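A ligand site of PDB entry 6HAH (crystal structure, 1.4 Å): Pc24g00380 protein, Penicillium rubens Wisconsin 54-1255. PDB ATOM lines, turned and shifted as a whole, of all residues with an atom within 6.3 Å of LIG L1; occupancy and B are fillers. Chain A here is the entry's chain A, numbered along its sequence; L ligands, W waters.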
ATOM      1  N   LYS A  11     -29.770  28.687  -4.483  1.00  0.00           N
ATOM      2  CA  LYS A  11     -28.511  29.050  -3.842  1.00  0.00           C
ATOM      3  C   LYS A  11     -28.359  28.474  -2.421  1.00  0.00           C
ATOM      4  O   LYS A  11     -27.278  28.617  -1.850  1.00  0.00           O
ATOM      5  CB  LYS A  11     -28.378  30.573  -3.827  1.00  0.00           C
ATOM      6  CG  LYS A  11     -28.314  31.137  -5.249  1.00  0.00           C
ATOM      7  CD  LYS A  11     -27.970  32.596  -5.278  1.00  0.00           C
ATOM      8  CE  LYS A  11     -29.180  33.476  -5.480  1.00  0.00           C
ATOM      9  NZ  LYS A  11     -28.807  34.885  -5.784  1.00  0.00           N
ATOM     10  N   ASN A  12     -29.422  27.884  -1.847  1.00  0.00           N
ATOM     11  CA  ASN A  12     -29.369  27.310  -0.500  1.00  0.00           C
ATOM     12  C   ASN A  12     -28.851  28.368   0.465  1.00  0.00           C
ATOM     13  O   ASN A  12     -27.917  28.120   1.212  1.00  0.00           O
ATOM     14  CB  ASN A  12     -28.513  26.042  -0.436  1.00  0.00           C
ATOM     15  CG  ASN A  12     -28.814  25.219   0.795  1.00  0.00           C
ATOM     16  OD1 ASN A  12     -29.887  25.358   1.429  1.00  0.00           O
ATOM     17  ND2 ASN A  12     -27.853  24.428   1.250  1.00  0.00           N
ATOM     18  N   LYS A  27     -25.045  31.338   4.021  1.00  0.00           N
ATOM     19  CA  LYS A  27     -25.312  29.998   3.531  1.00  0.00           C
ATOM     20  C   LYS A  27     -26.121  29.143   4.500  1.00  0.00           C
ATOM     21  O   LYS A  27     -25.782  29.030   5.685  1.00  0.00           O
ATOM     22  CB  LYS A  27     -23.998  29.274   3.239  1.00  0.00           C
ATOM     23  CG  LYS A  27     -23.255  29.824   2.021  1.00  0.00           C
ATOM     24  CD  LYS A  27     -21.938  29.130   1.782  1.00  0.00           C
ATOM     25  CE  LYS A  27     -20.995  29.984   0.953  1.00  0.00           C
ATOM     26  NZ  LYS A  27     -21.390  30.014  -0.481  1.00  0.00           N
ATOM     27  N   CYS A  28     -27.090  28.385   3.946  1.00  0.00           N
ATOM     28  CA  CYS A  28     -27.730  27.320   4.708  1.00  0.00           C
ATOM     29  C   CYS A  28     -26.724  26.175   4.792  1.00  0.00           C
ATOM     30  O   CYS A  28     -26.040  25.903   3.802  1.00  0.00           O
ATOM     31  CB  CYS A  28     -28.997  26.838   4.006  1.00  0.00           C
ATOM     32  SG  CYS A  28     -30.277  28.103   3.775  1.00  0.00           S
ATOM     33  N   PRO A  29     -26.822  25.352   5.839  1.00  0.00           N
ATOM     34  CA  PRO A  29     -26.051  24.096   5.842  1.00  0.00           C
ATOM     35  C   PRO A  29     -26.445  23.144   4.726  1.00  0.00           C
ATOM     36  O   PRO A  29     -27.546  23.176   4.186  1.00  0.00           O
ATOM     37  CB  PRO A  29     -26.356  23.498   7.217  1.00  0.00           C
ATOM     38  CG  PRO A  29     -26.766  24.680   8.062  1.00  0.00           C
ATOM     39  CD  PRO A  29     -27.527  25.563   7.122  1.00  0.00           C
ATOM     40  N   LYS A  30     -25.516  22.258   4.379  1.00  0.00           N
ATOM     41  CA  LYS A  30     -25.786  21.187   3.438  1.00  0.00           C
ATOM     42  C   LYS A  30     -26.603  20.053   4.079  1.00  0.00           C
ATOM     43  O   LYS A  30     -27.178  19.246   3.355  1.00  0.00           O
ATOM     44  CB  LYS A  30     -24.457  20.631   2.900  1.00  0.00           C
ATOM     45  CG  LYS A  30     -23.704  21.603   2.007  1.00  0.00           C
ATOM     46  CD  LYS A  30     -22.459  20.936   1.401  1.00  0.00           C
ATOM     47  CE  LYS A  30     -21.663  21.895   0.540  1.00  0.00           C
ATOM     48  NZ  LYS A  30     -22.437  22.340  -0.646  1.00  0.00           N
ATOM     49  N   PHE A  31     -26.558  19.921   5.412  1.00  0.00           N
ATOM     50  CA  PHE A  31     -27.248  18.843   6.119  1.00  0.00           C
ATOM     51  C   PHE A  31     -28.746  18.839   5.757  1.00  0.00           C
ATOM     52  O   PHE A  31     -29.368  19.902   5.647  1.00  0.00           O
ATOM     53  CB  PHE A  31     -27.098  19.025   7.641  1.00  0.00           C
ATOM     54  CG  PHE A  31     -25.815  18.524   8.262  1.00  0.00           C
ATOM     55  CD1 PHE A  31     -24.733  18.152   7.479  1.00  0.00           C
ATOM     56  CD2 PHE A  31     -25.669  18.478   9.636  1.00  0.00           C
ATOM     57  CE1 PHE A  31     -23.529  17.767   8.061  1.00  0.00           C
ATOM     58  CE2 PHE A  31     -24.491  18.042  10.220  1.00  0.00           C
ATOM     59  CZ  PHE A  31     -23.423  17.704   9.432  1.00  0.00           C
ATOM     60  N   ASP A  32     -29.328  17.642   5.704  1.00  0.00           N
ATOM     61  CA  ASP A  32     -30.714  17.427   5.274  1.00  0.00           C
ATOM     62  C   ASP A  32     -31.746  18.286   5.980  1.00  0.00           C
ATOM     63  O   ASP A  32     -32.664  18.775   5.330  1.00  0.00           O
ATOM     64  CB  ASP A  32     -31.093  15.954   5.495  1.00  0.00           C
ATOM     65  CG  ASP A  32     -30.222  15.004   4.711  1.00  0.00           C
ATOM     66  OD1 ASP A  32     -29.376  15.474   3.907  1.00  0.00           O
ATOM     67  OD2 ASP A  32     -30.347  13.767   4.935  1.00  0.00           O
ATOM     68  N   LYS A  34     -31.287  21.091   7.696  1.00  0.00           N
ATOM     69  CA  LYS A  34     -30.957  22.508   7.800  1.00  0.00           C
ATOM     70  C   LYS A  34     -30.858  23.198   6.428  1.00  0.00           C
ATOM     71  O   LYS A  34     -30.624  24.409   6.383  1.00  0.00           O
ATOM     72  CB  LYS A  34     -29.645  22.676   8.582  1.00  0.00           C
ATOM     73  CG  LYS A  34     -29.688  22.107  10.007  1.00  0.00           C
ATOM     74  CD  LYS A  34     -28.377  22.371  10.759  1.00  0.00           C
ATOM     75  CE  LYS A  34     -28.411  23.620  11.618  1.00  0.00           C
ATOM     76  NZ  LYS A  34     -27.151  24.413  11.566  1.00  0.00           N
ATOM     77  N   ASN A  50     -23.373  31.976  15.289  1.00  0.00           N
ATOM     78  CA  ASN A  50     -23.082  31.937  13.853  1.00  0.00           C
ATOM     79  C   ASN A  50     -23.609  30.628  13.243  1.00  0.00           C
ATOM     80  O   ASN A  50     -22.845  29.927  12.572  1.00  0.00           O
ATOM     81  CB  ASN A  50     -21.589  32.085  13.579  1.00  0.00           C
ATOM     82  CG  ASN A  50     -21.269  32.511  12.162  1.00  0.00           C
ATOM     83  OD1 ASN A  50     -22.083  33.146  11.482  1.00  0.00           O
ATOM     84  ND2 ASN A  50     -20.091  32.138  11.667  1.00  0.00           N
ATOM     85  N   ALA A  51     -24.859  30.230  13.585  1.00  0.00           N
ATOM     86  CA  ALA A  51     -25.454  28.973  13.141  1.00  0.00           C
ATOM     87  C   ALA A  51     -26.723  29.257  12.332  1.00  0.00           C
ATOM     88  O   ALA A  51     -27.509  30.127  12.690  1.00  0.00           O
ATOM     89  CB  ALA A  51     -25.822  28.114  14.359  1.00  0.00           C
ATOM     90  N   VAL A  52     -26.878  28.561  11.217  1.00  0.00           N
ATOM     91  CA  VAL A  52     -27.992  28.787  10.294  1.00  0.00           C
ATOM     92  C   VAL A  52     -28.841  27.538  10.183  1.00  0.00           C
ATOM     93  O   VAL A  52     -28.297  26.441  10.210  1.00  0.00           O
ATOM     94  CB  VAL A  52     -27.466  29.210   8.894  1.00  0.00           C
ATOM     95  CG1 VAL A  52     -28.636  29.459   7.916  1.00  0.00           C
ATOM     96  CG2 VAL A  52     -26.592  30.447   9.003  1.00  0.00           C
ATOM     97  N   ASP A  53     -30.182  27.704  10.206  1.00  0.00           N
ATOM     98  CA  ASP A  53     -31.067  26.579  10.038  1.00  0.00           C
ATOM     99  C   ASP A  53     -32.134  26.988   9.027  1.00  0.00           C
ATOM    100  O   ASP A  53     -32.963  27.840   9.342  1.00  0.00           O
ATOM    101  CB  ASP A  53     -31.697  26.221  11.400  1.00  0.00           C
ATOM    102  CG  ASP A  53     -32.656  25.043  11.376  1.00  0.00           C
ATOM    103  OD1 ASP A  53     -33.039  24.629  10.293  1.00  0.00           O
ATOM    104  OD2 ASP A  53     -33.007  24.531  12.470  1.00  0.00           O
HETATM  105  C1  LIG L   1     -23.056  25.744   7.599  1.00  0.00           C
HETATM  106  C2  LIG L   1     -22.851  25.149   6.359  1.00  0.00           C
HETATM  107  C3  LIG L   1     -22.805  23.751   6.283  1.00  0.00           C
HETATM  108  C4  LIG L   1     -22.930  22.945   7.402  1.00  0.00           C
HETATM  109  C5  LIG L   1     -23.182  23.558   8.640  1.00  0.00           C
HETATM  110  C6  LIG L   1     -23.247  24.963   8.729  1.00  0.00           C
HETATM  111  C7  LIG L   1     -22.890  26.022   5.116  1.00  0.00           C
HETATM  112  C8  LIG L   1     -21.503  26.336   4.591  1.00  0.00           C
HETATM  113  C9  LIG L   1     -20.897  27.548   4.935  1.00  0.00           C
HETATM  114  C10 LIG L   1     -19.653  27.866   4.376  1.00  0.00           C
HETATM  115  C11 LIG L   1     -19.003  26.920   3.583  1.00  0.00           C
HETATM  116  C12 LIG L   1     -19.626  25.739   3.219  1.00  0.00           C
HETATM  117  C13 LIG L   1     -18.895  24.691   2.385  1.00  0.00           C
HETATM  118  C14 LIG L   1     -23.043  21.433   7.228  1.00  0.00           C
HETATM  119  C15 LIG L   1     -21.724  20.696   7.116  1.00  0.00           C
HETATM  120  C16 LIG L   1     -21.321  19.948   8.215  1.00  0.00           C
HETATM  121  C17 LIG L   1     -19.568  18.875   6.930  1.00  0.00           C
HETATM  122  C18 LIG L   1     -21.082  20.461   5.899  1.00  0.00           C
HETATM  123  C19 LIG L   1     -20.274  19.045   8.138  1.00  0.00           C
HETATM  124  C20 LIG L   1     -20.027  19.546   5.787  1.00  0.00           C
HETATM  125  C21 LIG L   1     -19.941  18.700   3.329  1.00  0.00           C
HETATM  126  C22 LIG L   1     -21.124  17.986   3.475  1.00  0.00           C
HETATM  127  C23 LIG L   1     -20.855  25.417   3.794  1.00  0.00           C
HETATM  128  C24 LIG L   1     -19.282  19.482   4.465  1.00  0.00           C
HETATM  129  C25 LIG L   1     -21.669  17.248   2.414  1.00  0.00           C
HETATM  130  C26 LIG L   1     -21.003  17.251   1.187  1.00  0.00           C
HETATM  131  C27 LIG L   1     -19.849  18.022   1.012  1.00  0.00           C
HETATM  132  C28 LIG L   1     -19.282  18.674   2.102  1.00  0.00           C
HETATM  133  C29 LIG L   1     -19.108  17.935  -0.317  1.00  0.00           C
HETATM  134  C30 LIG L   1     -19.223  24.688   0.893  1.00  0.00           C
HETATM  135  C31 LIG L   1     -18.596  23.727   0.106  1.00  0.00           C
HETATM  136  C32 LIG L   1     -18.906  23.618  -1.251  1.00  0.00           C
HETATM  137  C33 LIG L   1     -19.704  24.607  -1.849  1.00  0.00           C
HETATM  138  C34 LIG L   1     -20.342  25.595  -1.071  1.00  0.00           C
HETATM  139  C35 LIG L   1     -20.022  25.677   0.295  1.00  0.00           C
HETATM  140  C36 LIG L   1     -19.418  19.084  -1.254  1.00  0.00           C
HETATM  141  C37 LIG L   1     -20.305  18.832  -2.303  1.00  0.00           C
HETATM  142  C38 LIG L   1     -20.585  19.822  -3.252  1.00  0.00           C
HETATM  143  C39 LIG L   1     -19.910  21.029  -3.184  1.00  0.00           C
HETATM  144  C40 LIG L   1     -18.989  21.276  -2.181  1.00  0.00           C
HETATM  145  C41 LIG L   1     -18.710  20.285  -1.232  1.00  0.00           C
HETATM  146  O1  LIG L   1     -17.745  22.870   0.737  1.00  0.00           O
HETATM  147  O2  LIG L   1     -21.487  24.326   3.326  1.00  0.00           O
HETATM  148  O3  LIG L   1     -22.760  23.149   5.074  1.00  0.00           O
HETATM  149  O4  LIG L   1     -21.479  21.067   4.765  1.00  0.00           O
HETATM  150  O5  LIG L   1     -18.195  19.448   1.972  1.00  0.00           O
HETATM  151  O6  LIG L   1     -17.745  20.535  -0.319  1.00  0.00           O
HETATM  152  S1  LIG L   1     -21.239  26.734  -1.794  1.00  0.00           S
HETATM  153  S2  LIG L   1     -18.981  29.295   4.653  1.00  0.00           S
HETATM  154  S3  LIG L   1     -23.574  25.691  10.129  1.00  0.00           S
HETATM  155  S4  LIG L   1     -19.790  18.303   9.486  1.00  0.00           S
HETATM  156  S5  LIG L   1     -22.979  16.335   2.633  1.00  0.00           S
HETATM  157  S6  LIG L   1     -21.707  19.583  -4.374  1.00  0.00           S
HETATM  158  C42 LIG L   1     -18.241  22.589  -2.162  1.00  0.00           C
HETATM  159  O7  LIG L   1     -20.366  27.920  -1.942  1.00  0.00           O
HETATM  160  O8  LIG L   1     -22.374  27.102  -0.925  1.00  0.00           O
HETATM  161  O9  LIG L   1     -21.749  26.235  -3.074  1.00  0.00           O
HETATM  162  O10 LIG L   1     -17.539  29.256   4.314  1.00  0.00           O
HETATM  163  O11 LIG L   1     -19.665  30.319   3.830  1.00  0.00           O
HETATM  164  O12 LIG L   1     -19.128  29.688   6.069  1.00  0.00           O
HETATM  165  O13 LIG L   1     -22.335  26.247  10.680  1.00  0.00           O
HETATM  166  O14 LIG L   1     -24.597  26.781   9.980  1.00  0.00           O
HETATM  167  O15 LIG L   1     -24.057  24.665  11.086  1.00  0.00           O
HETATM  168  O16 LIG L   1     -18.419  18.725   9.785  1.00  0.00           O
HETATM  169  O17 LIG L   1     -19.756  16.861   9.194  1.00  0.00           O
HETATM  170  O18 LIG L   1     -20.672  18.670  10.619  1.00  0.00           O
HETATM  171  O19 LIG L   1     -22.537  15.101   3.304  1.00  0.00           O
HETATM  172  O20 LIG L   1     -23.591  15.948   1.341  1.00  0.00           O
HETATM  173  O21 LIG L   1     -23.956  17.053   3.457  1.00  0.00           O
HETATM  174  O22 LIG L   1     -22.234  20.890  -4.827  1.00  0.00           O
HETATM  175  O23 LIG L   1     -22.817  18.789  -3.798  1.00  0.00           O
HETATM  176  O24 LIG L   1     -21.105  18.849  -5.507  1.00  0.00           O
HETATM  177  O1  LG2 L   2     -19.022  24.243   7.768  1.00  0.00           O
HETATM  178  C1  LG2 L   2     -17.948  23.462   7.249  1.00  0.00           C
HETATM  179  C2  LG2 L   2     -18.006  23.495   5.722  1.00  0.00           C
HETATM  180  O2  LG2 L   2     -17.085  22.557   5.154  1.00  0.00           O
HETATM  181  C3  LG2 L   2     -15.757  23.087   5.002  1.00  0.00           C
HETATM  182  C4  LG2 L   2     -15.327  23.091   3.543  1.00  0.00           C
HETATM  183  O3  LG2 L   2     -14.609  24.300   3.265  1.00  0.00           O
HETATM  184  C5  LG2 L   2     -15.051  24.919   2.058  1.00  0.00           C
HETATM  185  C6  LG2 L   2     -15.387  26.398   2.287  1.00  0.00           C
HETATM  186  O4  LG2 L   2     -15.843  26.961   1.056  1.00  0.00           O
HETATM  187  C7  LG2 L   2     -16.388  28.270   1.217  1.00  0.00           C
HETATM  188  C8  LG2 L   2     -16.887  28.776  -0.116  1.00  0.00           C
HETATM  189  O   HOH W   1     -24.808  27.764  -1.473  1.00  0.00           O
HETATM  190  O   HOH W   2     -15.412  19.520  -1.014  1.00  0.00           O
HETATM  191  O   HOH W   3     -15.973  19.191   3.399  1.00  0.00           O
HETATM  192  O   HOH W   4     -23.852  20.159  -1.595  1.00  0.00           O
HETATM  193  O   HOH W   5     -22.013  27.694  -5.473  1.00  0.00           O
HETATM  194  O   HOH W   6     -24.931  15.393  -0.913  1.00  0.00           O
HETATM  195  O   HOH W   7     -16.761  20.505   8.362  1.00  0.00           O
HETATM  196  O   HOH W   8     -22.613  23.774  -2.941  1.00  0.00           O
HETATM  197  O   HOH W   9     -24.079  25.505   2.032  1.00  0.00           O
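Cys 28 touches LIG L1.
Pro 29 touches LIG L1.
Phe 31 touches LIG L1.
Ala 51 touches LIG L1.
Hydrophobic or aromatic side chains within 4 Å of LIG L1: Pro 29, Phe 31 and Val 52.
Of the 13 residues printed, 8 come within 4 Å of LIG L1.
NZ of Lys 34 lies within hydrogen-bond range of O of Val 52.
The backbone NH (N) of Cys 28 is in hydrogen-bond range of the backbone carbonyl oxygen (O) of Asn 12 (2.9 Å).
The side-chain amide nitrogen (ND2) of Asn 12 lies within hydrogen-bond range of the backbone carbonyl oxygen (O) of Pro 29 (3.2 Å).
Water W1 lies within hydrogen-bond range of an oxygen (O8) of LIG L1 (2.6 Å) and the backbone carbonyl oxygen of Lys 11 (2.6 Å).
Water W8 lies within hydrogen-bond range of O9 of LIG L1 and NZ of Lys 30.
Water W4 lies within hydrogen-bond range of NZ of Lys 30 (2.8 Å) and O23 of LIG L1 (2.8 Å).
Water W9 lies within hydrogen-bond range of the backbone carbonyl oxygen of Cys 28 (2.7 Å) and an oxygen (O2) of LIG L1 (3.1 Å).
O3 of LIG L1 is in hydrogen-bond range of N of Lys 30.
N of Val 52 lies within hydrogen-bond range of O14 of LIG L1, at 3.1 Å.
NZ of Lys 27 lies within salt-bridge range of O7 of LIG L1, at 2.8 Å.
NZ of Lys 34 is in salt-bridge range of O15 of LIG L1, at 3.1 Å.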
